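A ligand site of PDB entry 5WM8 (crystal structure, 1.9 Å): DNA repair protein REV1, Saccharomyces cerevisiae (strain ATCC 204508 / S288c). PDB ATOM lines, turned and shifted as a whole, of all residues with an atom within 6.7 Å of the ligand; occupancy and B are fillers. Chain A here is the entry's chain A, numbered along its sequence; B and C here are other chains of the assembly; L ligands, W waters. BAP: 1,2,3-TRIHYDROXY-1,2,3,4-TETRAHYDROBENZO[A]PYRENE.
Residues that only touch the ligand: Lys 377, His 251 and Met 381. Within 4 Å of the ligand: Asp 95, Trp 113, His 251, Lys 377, Met 381 and DG 5 of chain B.
N2 of DG 5 of chain B is bonded to C4' of the ligand (1.3 Å). O3' of the ligand sits at hydrogen-bond distance from NE1 of Trp 113, 3.0 Å away. O3' of the ligand is in hydrogen-bond range of OD1 of Asp 95, 3.2 Å away.
N7 of DG 5 of chain B lies within hydrogen-bond range of the backbone NH (N) of Met 381, at 3.0 Å. O6 of DG 5 of chain B sits at hydrogen-bond distance from N of Gly 382, 3.0 Å away. The side-chain carboxylate (OD1) of Asp 95 lies close to the indole nitrogen (NE1) of Trp 113, at 3.3 Å. OD1 of Asp 95 lies within salt-bridge range of NZ of Lys 377, at 2.9 Å. The backbone NH of Asp 95 lies within hydrogen-bond range of OP1 of DC 4 of chain B (3.1 Å). OP1 of DC 4 of chain B lies within salt-bridge range of NZ of Lys 377. The side-chain amino group (NZ) of Lys 377 sits at hydrogen-bond distance from the backbone carbonyl oxygen (O) of Asn 93 (2.9 Å). OP2 of DT 10 of chain C sits at hydrogen-bond distance from the backbone NH of His 251 (3.3 Å).
Water W3 lies within hydrogen-bond range of OD2 of Asp 95 (2.8 Å), O3' of the ligand (3.0 Å) and N3 of DG 5 of chain B (3.2 Å). Water W1 bridges N1 of DG 5 of chain B (2.9 Å) and an oxygen (O2') of the ligand (3.1 Å). Water W2 bridges O of Gly 111 and OD2 of Asp 95.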
ATOM      1  N   ASN A  93      16.694 -28.822  -5.027  1.00  0.00           N
ATOM      2  CA  ASN A  93      16.787 -28.430  -6.446  1.00  0.00           C
ATOM      3  C   ASN A  93      15.472 -28.736  -7.202  1.00  0.00           C
ATOM      4  O   ASN A  93      15.488 -29.246  -8.319  1.00  0.00           O
ATOM      5  CB  ASN A  93      18.027 -29.088  -7.076  1.00  0.00           C
ATOM      6  CG  ASN A  93      19.325 -28.667  -6.358  1.00  0.00           C
ATOM      7  OD1 ASN A  93      19.329 -27.639  -5.668  1.00  0.00           O
ATOM      8  ND2 ASN A  93      20.403 -29.475  -6.468  1.00  0.00           N
ATOM      9  N   ASP A  95      11.805 -27.385  -8.710  1.00  0.00           N
ATOM     10  CA  ASP A  95      11.250 -26.205  -9.359  1.00  0.00           C
ATOM     11  C   ASP A  95      10.119 -25.643  -8.534  1.00  0.00           C
ATOM     12  O   ASP A  95       9.241 -26.383  -8.074  1.00  0.00           O
ATOM     13  CB  ASP A  95      10.652 -26.534 -10.753  1.00  0.00           C
ATOM     14  CG  ASP A  95      11.683 -26.582 -11.866  1.00  0.00           C
ATOM     15  OD1 ASP A  95      12.885 -26.728 -11.574  1.00  0.00           O
ATOM     16  OD2 ASP A  95      11.247 -26.502 -13.053  1.00  0.00           O
ATOM     17  N   GLY A 111       9.845 -21.043 -11.594  1.00  0.00           N
ATOM     18  CA  GLY A 111      10.932 -21.730 -12.283  1.00  0.00           C
ATOM     19  C   GLY A 111      12.273 -21.783 -11.553  1.00  0.00           C
ATOM     20  O   GLY A 111      13.132 -22.598 -11.901  1.00  0.00           O
ATOM     21  N   MET A 112      12.438 -20.920 -10.555  1.00  0.00           N
ATOM     22  CA  MET A 112      13.573 -20.930  -9.657  1.00  0.00           C
ATOM     23  C   MET A 112      13.539 -22.203  -8.802  1.00  0.00           C
ATOM     24  O   MET A 112      12.450 -22.663  -8.437  1.00  0.00           O
ATOM     25  CB  MET A 112      13.452 -19.685  -8.770  1.00  0.00           C
ATOM     26  CG  MET A 112      14.647 -19.346  -7.912  1.00  0.00           C
ATOM     27  SD  MET A 112      14.436 -17.748  -7.118  1.00  0.00           S
ATOM     28  CE  MET A 112      14.826 -16.611  -8.454  1.00  0.00           C
ATOM     29  N   TRP A 113      14.701 -22.779  -8.487  1.00  0.00           N
ATOM     30  CA  TRP A 113      14.741 -23.888  -7.512  1.00  0.00           C
ATOM     31  C   TRP A 113      14.551 -23.358  -6.121  1.00  0.00           C
ATOM     32  O   TRP A 113      14.936 -22.205  -5.833  1.00  0.00           O
ATOM     33  CB  TRP A 113      16.059 -24.668  -7.589  1.00  0.00           C
ATOM     34  CG  TRP A 113      16.316 -25.345  -8.897  1.00  0.00           C
ATOM     35  CD1 TRP A 113      15.468 -25.476  -9.970  1.00  0.00           C
ATOM     36  CD2 TRP A 113      17.515 -26.024  -9.255  1.00  0.00           C
ATOM     37  NE1 TRP A 113      16.073 -26.180 -10.980  1.00  0.00           N
ATOM     38  CE2 TRP A 113      17.329 -26.545 -10.564  1.00  0.00           C
ATOM     39  CE3 TRP A 113      18.739 -26.241  -8.617  1.00  0.00           C
ATOM     40  CZ2 TRP A 113      18.329 -27.259 -11.240  1.00  0.00           C
ATOM     41  CZ3 TRP A 113      19.729 -26.965  -9.292  1.00  0.00           C
ATOM     42  CH2 TRP A 113      19.508 -27.455 -10.584  1.00  0.00           C
ATOM     43  N   HIS A 251      14.317 -15.717 -23.089  1.00  0.00           N
ATOM     44  CA  HIS A 251      15.688 -15.424 -22.632  1.00  0.00           C
ATOM     45  C   HIS A 251      16.718 -15.238 -23.761  1.00  0.00           C
ATOM     46  O   HIS A 251      17.617 -14.402 -23.649  1.00  0.00           O
ATOM     47  CB  HIS A 251      16.184 -16.494 -21.633  1.00  0.00           C
ATOM     48  CG  HIS A 251      16.612 -17.780 -22.280  1.00  0.00           C
ATOM     49  ND1 HIS A 251      15.745 -18.841 -22.473  1.00  0.00           N
ATOM     50  CD2 HIS A 251      17.807 -18.179 -22.772  1.00  0.00           C
ATOM     51  CE1 HIS A 251      16.393 -19.828 -23.060  1.00  0.00           C
ATOM     52  NE2 HIS A 251      17.643 -19.454 -23.257  1.00  0.00           N
ATOM     53  N   MET A 365      18.235 -36.907 -25.799  1.00  0.00           N
ATOM     54  CA  MET A 365      19.159 -36.053 -25.087  1.00  0.00           C
ATOM     55  C   MET A 365      20.231 -36.955 -24.576  1.00  0.00           C
ATOM     56  O   MET A 365      19.950 -37.968 -23.938  1.00  0.00           O
ATOM     57  CB  MET A 365      18.466 -35.370 -23.898  1.00  0.00           C
ATOM     58  CG  MET A 365      17.397 -34.383 -24.325  1.00  0.00           C
ATOM     59  SD  MET A 365      18.060 -33.009 -25.261  1.00  0.00           S
ATOM     60  CE  MET A 365      18.394 -31.832 -23.958  1.00  0.00           C
ATOM     61  N   LYS A 377      20.171 -31.501 -10.056  1.00  0.00           N
ATOM     62  CA  LYS A 377      18.753 -31.918  -9.863  1.00  0.00           C
ATOM     63  C   LYS A 377      18.632 -33.429  -9.923  1.00  0.00           C
ATOM     64  O   LYS A 377      18.888 -34.013 -10.992  1.00  0.00           O
ATOM     65  CB  LYS A 377      17.829 -31.322 -10.945  1.00  0.00           C
ATOM     66  CG  LYS A 377      16.331 -31.594 -10.713  1.00  0.00           C
ATOM     67  CD  LYS A 377      15.471 -31.205 -11.903  1.00  0.00           C
ATOM     68  CE  LYS A 377      15.238 -29.707 -12.081  1.00  0.00           C
ATOM     69  NZ  LYS A 377      14.395 -29.140 -10.993  1.00  0.00           N
ATOM     70  N   MET A 381      18.012 -34.518 -16.432  1.00  0.00           N
ATOM     71  CA  MET A 381      18.829 -34.730 -17.630  1.00  0.00           C
ATOM     72  C   MET A 381      20.208 -34.056 -17.551  1.00  0.00           C
ATOM     73  O   MET A 381      21.183 -34.550 -18.120  1.00  0.00           O
ATOM     74  CB  MET A 381      18.095 -34.266 -18.902  1.00  0.00           C
ATOM     75  CG  MET A 381      17.740 -32.790 -18.973  1.00  0.00           C
ATOM     76  SD  MET A 381      17.101 -32.383 -20.586  1.00  0.00           S
ATOM     77  CE  MET A 381      16.185 -30.893 -20.203  1.00  0.00           C
ATOM     78  N   GLY A 382      20.297 -32.941 -16.815  1.00  0.00           N
ATOM     79  CA  GLY A 382      21.515 -32.112 -16.821  1.00  0.00           C
ATOM     80  C   GLY A 382      21.814 -31.514 -18.188  1.00  0.00           C
ATOM     81  O   GLY A 382      20.915 -31.415 -19.023  1.00  0.00           O
ATOM     82  P    DC B   4      11.224 -30.947  -9.630  1.00  0.00           P
ATOM     83  OP1  DC B   4      11.745 -29.878 -10.515  1.00  0.00           O
ATOM     84  OP2  DC B   4      10.406 -30.632  -8.446  1.00  0.00           O
ATOM     85  O5'  DC B   4      10.372 -31.972 -10.528  1.00  0.00           O
ATOM     86  C5'  DC B   4      10.914 -32.683 -11.656  1.00  0.00           C
ATOM     87  C4'  DC B   4       9.979 -33.805 -12.054  1.00  0.00           C
ATOM     88  O4'  DC B   4      10.006 -34.875 -11.089  1.00  0.00           O
ATOM     89  C3'  DC B   4       8.499 -33.425 -12.174  1.00  0.00           C
ATOM     90  O3'  DC B   4       8.164 -33.008 -13.499  1.00  0.00           O
ATOM     91  C2'  DC B   4       7.780 -34.737 -11.901  1.00  0.00           C
ATOM     92  C1'  DC B   4       8.836 -35.659 -11.299  1.00  0.00           C
ATOM     93  N1   DC B   4       8.451 -36.272 -10.023  1.00  0.00           N
ATOM     94  C2   DC B   4       8.093 -37.623  -9.986  1.00  0.00           C
ATOM     95  O2   DC B   4       8.095 -38.277 -11.047  1.00  0.00           O
ATOM     96  N3   DC B   4       7.753 -38.193  -8.812  1.00  0.00           N
ATOM     97  C4   DC B   4       7.740 -37.452  -7.698  1.00  0.00           C
ATOM     98  N4   DC B   4       7.388 -38.051  -6.557  1.00  0.00           N
ATOM     99  C5   DC B   4       8.090 -36.065  -7.703  1.00  0.00           C
ATOM    100  C6   DC B   4       8.446 -35.527  -8.873  1.00  0.00           C
ATOM    101  P    DG B   5       8.180 -31.471 -13.937  1.00  0.00           P
ATOM    102  OP1  DG B   5       8.066 -30.603 -12.735  1.00  0.00           O
ATOM    103  OP2  DG B   5       7.233 -31.322 -15.048  1.00  0.00           O
ATOM    104  O5'  DG B   5       9.652 -31.245 -14.518  1.00  0.00           O
ATOM    105  C5'  DG B   5      10.180 -32.089 -15.550  1.00  0.00           C
ATOM    106  C4'  DG B   5      10.888 -31.252 -16.594  1.00  0.00           C
ATOM    107  O4'  DG B   5      12.111 -30.698 -16.066  1.00  0.00           O
ATOM    108  C3'  DG B   5      11.328 -32.018 -17.832  1.00  0.00           C
ATOM    109  O3'  DG B   5      10.247 -32.065 -18.750  1.00  0.00           O
ATOM    110  C2'  DG B   5      12.451 -31.147 -18.373  1.00  0.00           C
ATOM    111  C1'  DG B   5      13.031 -30.499 -17.122  1.00  0.00           C
ATOM    112  N9   DG B   5      14.310 -31.032 -16.675  1.00  0.00           N
ATOM    113  C8   DG B   5      14.665 -32.347 -16.516  1.00  0.00           C
ATOM    114  N7   DG B   5      15.874 -32.500 -16.024  1.00  0.00           N
ATOM    115  C5   DG B   5      16.321 -31.200 -15.843  1.00  0.00           C
ATOM    116  C6   DG B   5      17.566 -30.721 -15.338  1.00  0.00           C
ATOM    117  O6   DG B   5      18.549 -31.374 -14.964  1.00  0.00           O
ATOM    118  N1   DG B   5      17.614 -29.327 -15.335  1.00  0.00           N
ATOM    119  C2   DG B   5      16.588 -28.507 -15.750  1.00  0.00           C
ATOM    120  N2   DG B   5      16.800 -27.176 -15.674  1.00  0.00           N
ATOM    121  N3   DG B   5      15.428 -28.945 -16.211  1.00  0.00           N
ATOM    122  C4   DG B   5      15.372 -30.287 -16.238  1.00  0.00           C
ATOM    123  P    DG C   8      20.399 -27.627 -31.083  1.00  0.00           P
ATOM    124  OP1  DG C   8      21.770 -27.187 -30.714  1.00  0.00           O
ATOM    125  OP2  DG C   8      19.787 -28.792 -30.388  1.00  0.00           O
ATOM    126  O5'  DG C   8      19.444 -26.364 -30.956  1.00  0.00           O
ATOM    127  C5'  DG C   8      19.511 -25.300 -31.919  1.00  0.00           C
ATOM    128  C4'  DG C   8      18.454 -24.271 -31.639  1.00  0.00           C
ATOM    129  O4'  DG C   8      17.211 -24.671 -32.255  1.00  0.00           O
ATOM    130  C3'  DG C   8      18.130 -24.061 -30.150  1.00  0.00           C
ATOM    131  O3'  DG C   8      17.898 -22.662 -29.973  1.00  0.00           O
ATOM    132  C2'  DG C   8      16.866 -24.881 -29.963  1.00  0.00           C
ATOM    133  C1'  DG C   8      16.176 -24.625 -31.292  1.00  0.00           C
ATOM    134  N9   DG C   8      15.133 -25.561 -31.693  1.00  0.00           N
ATOM    135  C8   DG C   8      15.145 -26.930 -31.618  1.00  0.00           C
ATOM    136  N7   DG C   8      14.058 -27.487 -32.096  1.00  0.00           N
ATOM    137  C5   DG C   8      13.276 -26.411 -32.498  1.00  0.00           C
ATOM    138  C6   DG C   8      11.988 -26.379 -33.082  1.00  0.00           C
ATOM    139  O6   DG C   8      11.240 -27.332 -33.370  1.00  0.00           O
ATOM    140  N1   DG C   8      11.564 -25.074 -33.336  1.00  0.00           N
ATOM    141  C2   DG C   8      12.305 -23.947 -33.053  1.00  0.00           C
ATOM    142  N2   DG C   8      11.733 -22.778 -33.368  1.00  0.00           N
ATOM    143  N3   DG C   8      13.514 -23.959 -32.524  1.00  0.00           N
ATOM    144  C4   DG C   8      13.938 -25.218 -32.267  1.00  0.00           C
ATOM    145  P    DG C   9      17.978 -21.981 -28.530  1.00  0.00           P
ATOM    146  OP1  DG C   9      19.127 -21.038 -28.536  1.00  0.00           O
ATOM    147  OP2  DG C   9      17.865 -23.020 -27.473  1.00  0.00           O
ATOM    148  O5'  DG C   9      16.662 -21.101 -28.485  1.00  0.00           O
ATOM    149  C5'  DG C   9      16.344 -20.195 -29.550  1.00  0.00           C
ATOM    150  C4'  DG C   9      14.911 -19.724 -29.416  1.00  0.00           C
ATOM    151  O4'  DG C   9      14.010 -20.732 -29.949  1.00  0.00           O
ATOM    152  C3'  DG C   9      14.457 -19.451 -27.987  1.00  0.00           C
ATOM    153  O3'  DG C   9      13.915 -18.129 -27.992  1.00  0.00           O
ATOM    154  C2'  DG C   9      13.476 -20.566 -27.677  1.00  0.00           C
ATOM    155  C1'  DG C   9      12.958 -20.999 -29.042  1.00  0.00           C
ATOM    156  N9   DG C   9      12.613 -22.414 -29.180  1.00  0.00           N
ATOM    157  C8   DG C   9      13.424 -23.483 -28.906  1.00  0.00           C
ATOM    158  N7   DG C   9      12.872 -24.631 -29.167  1.00  0.00           N
ATOM    159  C5   DG C   9      11.611 -24.301 -29.649  1.00  0.00           C
ATOM    160  C6   DG C   9      10.542 -25.134 -30.087  1.00  0.00           C
ATOM    161  O6   DG C   9      10.497 -26.365 -30.146  1.00  0.00           O
ATOM    162  N1   DG C   9       9.446 -24.376 -30.503  1.00  0.00           N
ATOM    163  C2   DG C   9       9.383 -23.007 -30.480  1.00  0.00           C
ATOM    164  N2   DG C   9       8.236 -22.457 -30.918  1.00  0.00           N
ATOM    165  N3   DG C   9      10.374 -22.221 -30.089  1.00  0.00           N
ATOM    166  C4   DG C   9      11.449 -22.933 -29.680  1.00  0.00           C
ATOM    167  P    DT C  10      13.481 -17.411 -26.653  1.00  0.00           P
ATOM    168  OP1  DT C  10      13.548 -15.947 -26.881  1.00  0.00           O
ATOM    169  OP2  DT C  10      14.190 -18.015 -25.502  1.00  0.00           O
ATOM    170  O5'  DT C  10      11.946 -17.814 -26.552  1.00  0.00           O
ATOM    171  C5'  DT C  10      10.996 -17.359 -27.520  1.00  0.00           C
ATOM    172  C4'  DT C  10       9.640 -17.938 -27.231  1.00  0.00           C
ATOM    173  O4'  DT C  10       9.662 -19.347 -27.529  1.00  0.00           O
ATOM    174  C3'  DT C  10       9.175 -17.822 -25.773  1.00  0.00           C
ATOM    175  O3'  DT C  10       8.197 -16.776 -25.739  1.00  0.00           O
ATOM    176  C2'  DT C  10       8.645 -19.219 -25.424  1.00  0.00           C
ATOM    177  C1'  DT C  10       8.658 -19.976 -26.745  1.00  0.00           C
ATOM    178  N1   DT C  10       8.992 -21.407 -26.680  1.00  0.00           N
ATOM    179  C2   DT C  10       8.107 -22.317 -27.212  1.00  0.00           C
ATOM    180  O2   DT C  10       7.015 -22.011 -27.652  1.00  0.00           O
ATOM    181  N3   DT C  10       8.529 -23.618 -27.145  1.00  0.00           N
ATOM    182  C4   DT C  10       9.732 -24.092 -26.639  1.00  0.00           C
ATOM    183  O4   DT C  10       9.976 -25.291 -26.686  1.00  0.00           O
ATOM    184  C5   DT C  10      10.621 -23.076 -26.146  1.00  0.00           C
ATOM    185  C7   DT C  10      11.957 -23.475 -25.588  1.00  0.00           C
ATOM    186  C6   DT C  10      10.219 -21.800 -26.186  1.00  0.00           C
HETATM  187  C1  BAP L   1      17.962 -24.216 -23.107  1.00  0.00           C
HETATM  188  C2  BAP L   1      17.592 -25.489 -23.554  1.00  0.00           C
HETATM  189  C3  BAP L   1      17.084 -26.478 -22.700  1.00  0.00           C
HETATM  190  C3A BAP L   1      16.916 -26.210 -21.342  1.00  0.00           C
HETATM  191  C4  BAP L   1      16.413 -27.144 -20.433  1.00  0.00           C
HETATM  192  C5  BAP L   1      16.261 -26.862 -19.069  1.00  0.00           C
HETATM  193  C5A BAP L   1      16.604 -25.600 -18.541  1.00  0.00           C
HETATM  194  C6  BAP L   1      16.471 -25.202 -17.113  1.00  0.00           C
HETATM  195  C7  BAP L   1      16.900 -23.831 -16.692  1.00  0.00           C
HETATM  196  C8  BAP L   1      17.390 -22.895 -17.605  1.00  0.00           C
HETATM  197  C8A BAP L   1      17.548 -23.209 -18.955  1.00  0.00           C
HETATM  198  C9  BAP L   1      18.041 -22.276 -19.884  1.00  0.00           C
HETATM  199  C10 BAP L   1      18.189 -22.592 -21.254  1.00  0.00           C
HETATM  200  C1A BAP L   1      17.836 -23.855 -21.771  1.00  0.00           C
HETATM  201  C3B BAP L   1      17.303 -24.875 -20.857  1.00  0.00           C
HETATM  202  C5B BAP L   1      17.152 -24.555 -19.440  1.00  0.00           C
HETATM  203  C1' BAP L   1      16.754 -23.404 -15.284  1.00  0.00           C
HETATM  204  O1' BAP L   1      15.631 -22.523 -15.280  1.00  0.00           O
HETATM  205  C2' BAP L   1      16.471 -24.504 -14.264  1.00  0.00           C
HETATM  206  O2' BAP L   1      17.672 -25.166 -13.859  1.00  0.00           O
HETATM  207  C3' BAP L   1      15.476 -25.515 -14.809  1.00  0.00           C
HETATM  208  O3' BAP L   1      15.178 -26.472 -13.784  1.00  0.00           O
HETATM  209  C4' BAP L   1      15.966 -26.215 -16.092  1.00  0.00           C
HETATM  210  O   HOH W   1      19.625 -27.494 -14.355  1.00  0.00           O
HETATM  211  O   HOH W   2      12.497 -24.027 -13.922  1.00  0.00           O
HETATM  212  O   HOH W   3      12.744 -27.672 -15.059  1.00  0.00           O
